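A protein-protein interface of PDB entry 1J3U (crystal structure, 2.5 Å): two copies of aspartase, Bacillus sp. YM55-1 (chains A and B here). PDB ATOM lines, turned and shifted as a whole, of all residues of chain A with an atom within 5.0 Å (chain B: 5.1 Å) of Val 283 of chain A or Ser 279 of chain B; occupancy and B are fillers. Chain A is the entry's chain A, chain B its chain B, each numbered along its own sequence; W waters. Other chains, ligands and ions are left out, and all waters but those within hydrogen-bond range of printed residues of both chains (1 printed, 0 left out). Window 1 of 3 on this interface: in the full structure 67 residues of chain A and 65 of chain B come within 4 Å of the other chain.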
ATOM      1  N   ASP A 211      -3.384  17.027 -10.099  1.00  0.00           N
ATOM      2  CA  ASP A 211      -4.708  17.623  -9.980  1.00  0.00           C
ATOM      3  C   ASP A 211      -5.520  16.721  -9.079  1.00  0.00           C
ATOM      4  O   ASP A 211      -6.218  17.188  -8.172  1.00  0.00           O
ATOM      5  CB  ASP A 211      -5.393  17.743 -11.340  1.00  0.00           C
ATOM      6  CG  ASP A 211      -5.012  19.010 -12.065  1.00  0.00           C
ATOM      7  OD1 ASP A 211      -4.765  20.031 -11.380  1.00  0.00           O
ATOM      8  OD2 ASP A 211      -4.973  18.991 -13.315  1.00  0.00           O
ATOM      9  N   ARG A 214      -4.753  17.625  -5.488  1.00  0.00           N
ATOM     10  CA  ARG A 214      -5.414  18.878  -5.105  1.00  0.00           C
ATOM     11  C   ARG A 214      -6.929  18.767  -4.972  1.00  0.00           C
ATOM     12  O   ARG A 214      -7.519  19.245  -4.000  1.00  0.00           O
ATOM     13  CB  ARG A 214      -5.099  19.986  -6.117  1.00  0.00           C
ATOM     14  CG  ARG A 214      -3.754  20.674  -5.933  1.00  0.00           C
ATOM     15  CD  ARG A 214      -3.591  21.811  -6.939  1.00  0.00           C
ATOM     16  NE  ARG A 214      -3.487  21.305  -8.302  1.00  0.00           N
ATOM     17  CZ  ARG A 214      -2.345  21.198  -8.972  1.00  0.00           C
ATOM     18  NH1 ARG A 214      -1.201  21.575  -8.405  1.00  0.00           N
ATOM     19  NH2 ARG A 214      -2.348  20.688 -10.196  1.00  0.00           N
ATOM     20  N   SER A 278     -13.994  24.701  -6.071  1.00  0.00           N
ATOM     21  CA  SER A 278     -14.026  25.320  -7.385  1.00  0.00           C
ATOM     22  C   SER A 278     -12.614  25.720  -7.802  1.00  0.00           C
ATOM     23  O   SER A 278     -12.259  25.640  -8.982  1.00  0.00           O
ATOM     24  CB  SER A 278     -14.936  26.552  -7.365  1.00  0.00           C
ATOM     25  OG  SER A 278     -15.048  27.115  -8.659  1.00  0.00           O
ATOM     26  N   SER A 279     -11.812  26.158  -6.835  1.00  0.00           N
ATOM     27  CA  SER A 279     -10.436  26.561  -7.116  1.00  0.00           C
ATOM     28  C   SER A 279      -9.647  25.374  -7.669  1.00  0.00           C
ATOM     29  O   SER A 279      -8.914  25.501  -8.648  1.00  0.00           O
ATOM     30  CB  SER A 279      -9.751  27.083  -5.838  1.00  0.00           C
ATOM     31  OG  SER A 279     -10.246  28.360  -5.452  1.00  0.00           O
ATOM     32  N   ALA A 280      -9.811  24.219  -7.032  1.00  0.00           N
ATOM     33  CA  ALA A 280      -9.123  23.007  -7.447  1.00  0.00           C
ATOM     34  C   ALA A 280      -9.583  22.509  -8.818  1.00  0.00           C
ATOM     35  O   ALA A 280      -8.785  21.951  -9.576  1.00  0.00           O
ATOM     36  CB  ALA A 280      -9.326  21.914  -6.403  1.00  0.00           C
ATOM     37  N   LEU A 281     -10.866  22.693  -9.126  1.00  0.00           N
ATOM     38  CA  LEU A 281     -11.405  22.258 -10.412  1.00  0.00           C
ATOM     39  C   LEU A 281     -10.902  23.180 -11.517  1.00  0.00           C
ATOM     40  O   LEU A 281     -10.488  22.720 -12.590  1.00  0.00           O
ATOM     41  CB  LEU A 281     -12.933  22.274 -10.392  1.00  0.00           C
ATOM     42  CG  LEU A 281     -13.611  21.386  -9.344  1.00  0.00           C
ATOM     43  CD1 LEU A 281     -15.124  21.552  -9.434  1.00  0.00           C
ATOM     44  CD2 LEU A 281     -13.209  19.929  -9.564  1.00  0.00           C
ATOM     45  N   LYS A 282     -10.934  24.485 -11.251  1.00  0.00           N
ATOM     46  CA  LYS A 282     -10.475  25.452 -12.235  1.00  0.00           C
ATOM     47  C   LYS A 282      -9.036  25.142 -12.608  1.00  0.00           C
ATOM     48  O   LYS A 282      -8.708  25.053 -13.787  1.00  0.00           O
ATOM     49  CB  LYS A 282     -10.569  26.873 -11.695  1.00  0.00           C
ATOM     50  CG  LYS A 282     -10.233  27.923 -12.735  1.00  0.00           C
ATOM     51  CD  LYS A 282      -9.115  28.840 -12.275  1.00  0.00           C
ATOM     52  CE  LYS A 282      -9.538  29.730 -11.128  1.00  0.00           C
ATOM     53  NZ  LYS A 282      -8.374  30.474 -10.582  1.00  0.00           N
ATOM     54  N   VAL A 283      -8.179  24.962 -11.610  1.00  0.00           N
ATOM     55  CA  VAL A 283      -6.774  24.661 -11.888  1.00  0.00           C
ATOM     56  C   VAL A 283      -6.653  23.431 -12.764  1.00  0.00           C
ATOM     57  O   VAL A 283      -5.927  23.428 -13.752  1.00  0.00           O
ATOM     58  CB  VAL A 283      -5.957  24.406 -10.613  1.00  0.00           C
ATOM     59  CG1 VAL A 283      -4.552  23.959 -11.002  1.00  0.00           C
ATOM     60  CG2 VAL A 283      -5.906  25.671  -9.763  1.00  0.00           C
ATOM     61  N   CYS A 284      -7.364  22.380 -12.394  1.00  0.00           N
ATOM     62  CA  CYS A 284      -7.314  21.168 -13.182  1.00  0.00           C
ATOM     63  C   CYS A 284      -7.673  21.482 -14.635  1.00  0.00           C
ATOM     64  O   CYS A 284      -6.933  21.132 -15.552  1.00  0.00           O
ATOM     65  CB  CYS A 284      -8.277  20.128 -12.630  1.00  0.00           C
ATOM     66  SG  CYS A 284      -8.359  18.693 -13.677  1.00  0.00           S
ATOM     67  N   MET A 285      -8.799  22.153 -14.852  1.00  0.00           N
ATOM     68  CA  MET A 285      -9.203  22.472 -16.215  1.00  0.00           C
ATOM     69  C   MET A 285      -8.190  23.353 -16.957  1.00  0.00           C
ATOM     70  O   MET A 285      -8.132  23.327 -18.188  1.00  0.00           O
ATOM     71  CB  MET A 285     -10.586  23.125 -16.222  1.00  0.00           C
ATOM     72  CG  MET A 285     -11.714  22.179 -15.843  1.00  0.00           C
ATOM     73  SD  MET A 285     -11.620  20.604 -16.724  1.00  0.00           S
ATOM     74  CE  MET A 285     -11.962  21.091 -18.410  1.00  0.00           C
ATOM     75  N   ILE A 286      -7.396  24.134 -16.228  1.00  0.00           N
ATOM     76  CA  ILE A 286      -6.391  24.966 -16.879  1.00  0.00           C
ATOM     77  C   ILE A 286      -5.383  24.018 -17.505  1.00  0.00           C
ATOM     78  O   ILE A 286      -5.042  24.127 -18.682  1.00  0.00           O
ATOM     79  CB  ILE A 286      -5.650  25.849 -15.883  1.00  0.00           C
ATOM     80  CG1 ILE A 286      -6.583  26.957 -15.386  1.00  0.00           C
ATOM     81  CG2 ILE A 286      -4.379  26.412 -16.541  1.00  0.00           C
ATOM     82  CD1 ILE A 286      -6.050  27.717 -14.170  1.00  0.00           C
ATOM     83  N   ASN A 287      -4.907  23.078 -16.701  1.00  0.00           N
ATOM     84  CA  ASN A 287      -3.965  22.099 -17.186  1.00  0.00           C
ATOM     85  C   ASN A 287      -4.615  21.358 -18.343  1.00  0.00           C
ATOM     86  O   ASN A 287      -4.054  21.291 -19.438  1.00  0.00           O
ATOM     87  CB  ASN A 287      -3.617  21.112 -16.086  1.00  0.00           C
ATOM     88  CG  ASN A 287      -3.219  21.792 -14.801  1.00  0.00           C
ATOM     89  OD1 ASN A 287      -2.449  22.750 -14.802  1.00  0.00           O
ATOM     90  ND2 ASN A 287      -3.732  21.291 -13.690  1.00  0.00           N
ATOM     91  N   ASP B 272       0.895  24.661 -13.287  1.00  0.00           N
ATOM     92  CA  ASP B 272      -0.176  24.438 -12.324  1.00  0.00           C
ATOM     93  C   ASP B 272       0.157  24.803 -10.872  1.00  0.00           C
ATOM     94  O   ASP B 272      -0.737  25.127 -10.091  1.00  0.00           O
ATOM     95  CB  ASP B 272      -0.645  22.981 -12.400  1.00  0.00           C
ATOM     96  CG  ASP B 272       0.421  22.002 -11.975  1.00  0.00           C
ATOM     97  OD1 ASP B 272       1.579  22.162 -12.407  1.00  0.00           O
ATOM     98  OD2 ASP B 272       0.096  21.063 -11.217  1.00  0.00           O
ATOM     99  N   THR B 275      -0.895  28.540 -10.275  1.00  0.00           N
ATOM    100  CA  THR B 275      -2.320  28.749 -10.174  1.00  0.00           C
ATOM    101  C   THR B 275      -2.818  28.196  -8.851  1.00  0.00           C
ATOM    102  O   THR B 275      -3.731  28.752  -8.251  1.00  0.00           O
ATOM    103  CB  THR B 275      -3.056  28.065 -11.325  1.00  0.00           C
ATOM    104  OG1 THR B 275      -2.648  26.691 -11.399  1.00  0.00           O
ATOM    105  CG2 THR B 275      -2.745  28.767 -12.641  1.00  0.00           C
ATOM    106  N   GLU B 276      -2.223  27.106  -8.388  1.00  0.00           N
ATOM    107  CA  GLU B 276      -2.635  26.541  -7.112  1.00  0.00           C
ATOM    108  C   GLU B 276      -2.533  27.608  -6.028  1.00  0.00           C
ATOM    109  O   GLU B 276      -3.439  27.757  -5.196  1.00  0.00           O
ATOM    110  CB  GLU B 276      -1.763  25.353  -6.722  1.00  0.00           C
ATOM    111  CG  GLU B 276      -2.029  24.881  -5.312  1.00  0.00           C
ATOM    112  CD  GLU B 276      -1.335  23.588  -4.979  1.00  0.00           C
ATOM    113  OE1 GLU B 276      -1.520  23.107  -3.840  1.00  0.00           O
ATOM    114  OE2 GLU B 276      -0.616  23.043  -5.844  1.00  0.00           O
ATOM    115  N   VAL B 277      -1.434  28.353  -6.039  1.00  0.00           N
ATOM    116  CA  VAL B 277      -1.226  29.403  -5.053  1.00  0.00           C
ATOM    117  C   VAL B 277      -2.214  30.555  -5.233  1.00  0.00           C
ATOM    118  O   VAL B 277      -2.860  30.983  -4.275  1.00  0.00           O
ATOM    119  CB  VAL B 277       0.208  29.965  -5.124  1.00  0.00           C
ATOM    120  CG1 VAL B 277       0.362  31.129  -4.169  1.00  0.00           C
ATOM    121  CG2 VAL B 277       1.200  28.882  -4.776  1.00  0.00           C
ATOM    122  N   SER B 278      -2.333  31.055  -6.460  1.00  0.00           N
ATOM    123  CA  SER B 278      -3.241  32.163  -6.724  1.00  0.00           C
ATOM    124  C   SER B 278      -4.633  31.798  -6.252  1.00  0.00           C
ATOM    125  O   SER B 278      -5.314  32.607  -5.623  1.00  0.00           O
ATOM    126  CB  SER B 278      -3.281  32.507  -8.219  1.00  0.00           C
ATOM    127  OG  SER B 278      -4.110  33.640  -8.459  1.00  0.00           O
ATOM    128  N   SER B 279      -5.048  30.575  -6.548  1.00  0.00           N
ATOM    129  CA  SER B 279      -6.368  30.117  -6.157  1.00  0.00           C
ATOM    130  C   SER B 279      -6.575  30.154  -4.640  1.00  0.00           C
ATOM    131  O   SER B 279      -7.677  30.441  -4.174  1.00  0.00           O
ATOM    132  CB  SER B 279      -6.616  28.705  -6.696  1.00  0.00           C
ATOM    133  OG  SER B 279      -6.734  28.739  -8.109  1.00  0.00           O
ATOM    134  N   ALA B 280      -5.524  29.868  -3.874  1.00  0.00           N
ATOM    135  CA  ALA B 280      -5.636  29.886  -2.416  1.00  0.00           C
ATOM    136  C   ALA B 280      -5.756  31.317  -1.915  1.00  0.00           C
ATOM    137  O   ALA B 280      -6.571  31.610  -1.038  1.00  0.00           O
ATOM    138  CB  ALA B 280      -4.432  29.223  -1.784  1.00  0.00           C
ATOM    139  N   LEU B 281      -4.937  32.202  -2.480  1.00  0.00           N
ATOM    140  CA  LEU B 281      -4.938  33.618  -2.122  1.00  0.00           C
ATOM    141  C   LEU B 281      -6.280  34.238  -2.494  1.00  0.00           C
ATOM    142  O   LEU B 281      -6.755  35.157  -1.818  1.00  0.00           O
ATOM    143  CB  LEU B 281      -3.833  34.380  -2.871  1.00  0.00           C
ATOM    144  CG  LEU B 281      -2.401  33.852  -2.892  1.00  0.00           C
ATOM    145  CD1 LEU B 281      -1.519  34.815  -3.672  1.00  0.00           C
ATOM    146  CD2 LEU B 281      -1.897  33.683  -1.472  1.00  0.00           C
ATOM    147  N   LYS B 282      -6.885  33.754  -3.578  1.00  0.00           N
ATOM    148  CA  LYS B 282      -8.174  34.291  -4.001  1.00  0.00           C
ATOM    149  C   LYS B 282      -9.200  33.908  -2.941  1.00  0.00           C
ATOM    150  O   LYS B 282      -9.880  34.773  -2.395  1.00  0.00           O
ATOM    151  CB  LYS B 282      -8.576  33.734  -5.363  1.00  0.00           C
ATOM    152  CG  LYS B 282      -9.763  34.425  -5.997  1.00  0.00           C
ATOM    153  CD  LYS B 282     -10.806  33.407  -6.466  1.00  0.00           C
ATOM    154  CE  LYS B 282     -10.255  32.443  -7.524  1.00  0.00           C
ATOM    155  NZ  LYS B 282     -10.880  31.078  -7.488  1.00  0.00           N
ATOM    156  N   VAL B 283      -9.291  32.618  -2.633  1.00  0.00           N
ATOM    157  CA  VAL B 283     -10.229  32.153  -1.628  1.00  0.00           C
ATOM    158  C   VAL B 283     -10.058  32.958  -0.344  1.00  0.00           C
ATOM    159  O   VAL B 283     -11.046  33.316   0.303  1.00  0.00           O
ATOM    160  CB  VAL B 283     -10.040  30.652  -1.327  1.00  0.00           C
ATOM    161  CG1 VAL B 283     -10.754  30.270  -0.045  1.00  0.00           C
ATOM    162  CG2 VAL B 283     -10.587  29.822  -2.491  1.00  0.00           C
ATOM    163  N   ASP B 344      -5.931  36.861 -10.348  1.00  0.00           N
ATOM    164  CA  ASP B 344      -6.162  35.426 -10.530  1.00  0.00           C
ATOM    165  C   ASP B 344      -6.747  35.079 -11.919  1.00  0.00           C
ATOM    166  O   ASP B 344      -6.634  33.947 -12.385  1.00  0.00           O
ATOM    167  CB  ASP B 344      -7.059  34.877  -9.408  1.00  0.00           C
ATOM    168  CG  ASP B 344      -7.398  33.392  -9.589  1.00  0.00           C
ATOM    169  OD1 ASP B 344      -8.432  33.091 -10.239  1.00  0.00           O
ATOM    170  OD2 ASP B 344      -6.641  32.525  -9.089  1.00  0.00           O
HETATM  171  O   HOH W   1       0.613  22.774 -16.030  1.00  0.00           O
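Water W1 lies within hydrogen-bond range of OD1 of Asn 287 of chain A (3.3 Å) and N of Asp 272 of chain B (3.3 Å).
Ser 279 of chain B touches Ser 279 of chain A. Val 283 of chain B touches Ser 279 of chain A (CG2 to OG, 3.3 Å). Val 283 of chain A touches Thr 275 of chain B. OG of Ser 279 of chain B touches CG2 of Val 283 of chain A, at 3.6 Å. CD1 of Ile 286 of chain A touches CG2 of Thr 275 of chain B (3.8 Å). Asn 287 of chain A touches Asp 272 of chain B (OD1 to CB, 3.0 Å).
NH2 of Arg 214 of chain A lies within salt-bridge range of OD2 of Asp 272 of chain B (2.7 Å). The side-chain carboxylate of Asp 344 of chain B is in salt-bridge range of the side-chain amino group of Lys 282 of chain A, 2.6 Å away. NZ of Lys 282 of chain B is in hydrogen-bond range of OG of Ser 279 of chain A, 3.5 Å away. The guanidinium group of Arg 214 of chain A is in salt-bridge range of the side-chain carboxylate of Glu 276 of chain B. The side-chain amino group (NZ) of Lys 282 of chain A sits at hydrogen-bond distance from the side-chain hydroxyl (OG) of Ser 279 of chain B, at 3.4 Å.
Ser 279 of chain A touches its own counterpart, Ser 279 of chain B. Ser 279 of chain A touches Lys 282 of chain B, and with the chains exchanged Lys 282 of chain A touches Ser 279 of chain B. Ser 279 of chain A touches Val 283 of chain B, and with the chains exchanged Val 283 of chain A touches Ser 279 of chain B. Positions printed for both chains: 278, 279, 280, 281, 282 and 283.
Hydrophobic or aromatic side chains of chain A that line the printed part of chain B: Val 283 and Ile 286. Along chain A the printed residues that touch a printed residue of chain B span positions 214 to 287. Hydrophobic or aromatic side chains of chain B within 4 Å of the printed part of chain A: Val 283.
The side-chain hydroxyl of Ser 278 of chain B is in hydrogen-bond range of the side-chain carboxylate of Asp 344 of chain B. NH2 of Arg 214 of chain A lies within salt-bridge range of OD1 of Asp 211 of chain A. The backbone carbonyl oxygen (O) of Val 283 of chain A is in hydrogen-bond range of the side-chain amide nitrogen (ND2) of Asn 287 of chain A (3.1 Å). The side-chain amide nitrogen (ND2) of Asn 287 of chain A is in hydrogen-bond range of the side-chain carboxylate (OD2) of Asp 211 of chain A, at 2.6 Å. The backbone carbonyl oxygen (O) of Thr 275 of chain B lies within hydrogen-bond range of the side-chain hydroxyl (OG) of Ser 279 of chain B. O of Asp 272 of chain B lies within hydrogen-bond range of OG1 of Thr 275 of chain B, at 2.8 Å.
Of chain B, only Thr 275 (3.4 Å) and Ser 279 (3.6 Å) come within 4 Å of Val 283 of chain A. Of chain A, only Ser 279, Lys 282 and Val 283 come within 4 Å of Ser 279 of chain B. Of the printed residues of chain B, Asn 287 of chain A touches Asp 272. Of the printed residues of chain A, Thr 275 of chain B touches Val 283 (3.4 Å) and Ile 286 (3.8 Å). Of the printed residues of chain B, Ser 279 of chain A touches Ser 279 (3.5 Å), Lys 282 (3.5 Å) and Val 283 (3.3 Å). The nearest residue of chain B that does not touch Val 283 of chain A is Asp 272 of chain B (4.1 Å). The nearest printed residue of chain B that does not touch Asn 287 of chain A is Thr 275 of chain B (5.2 Å).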
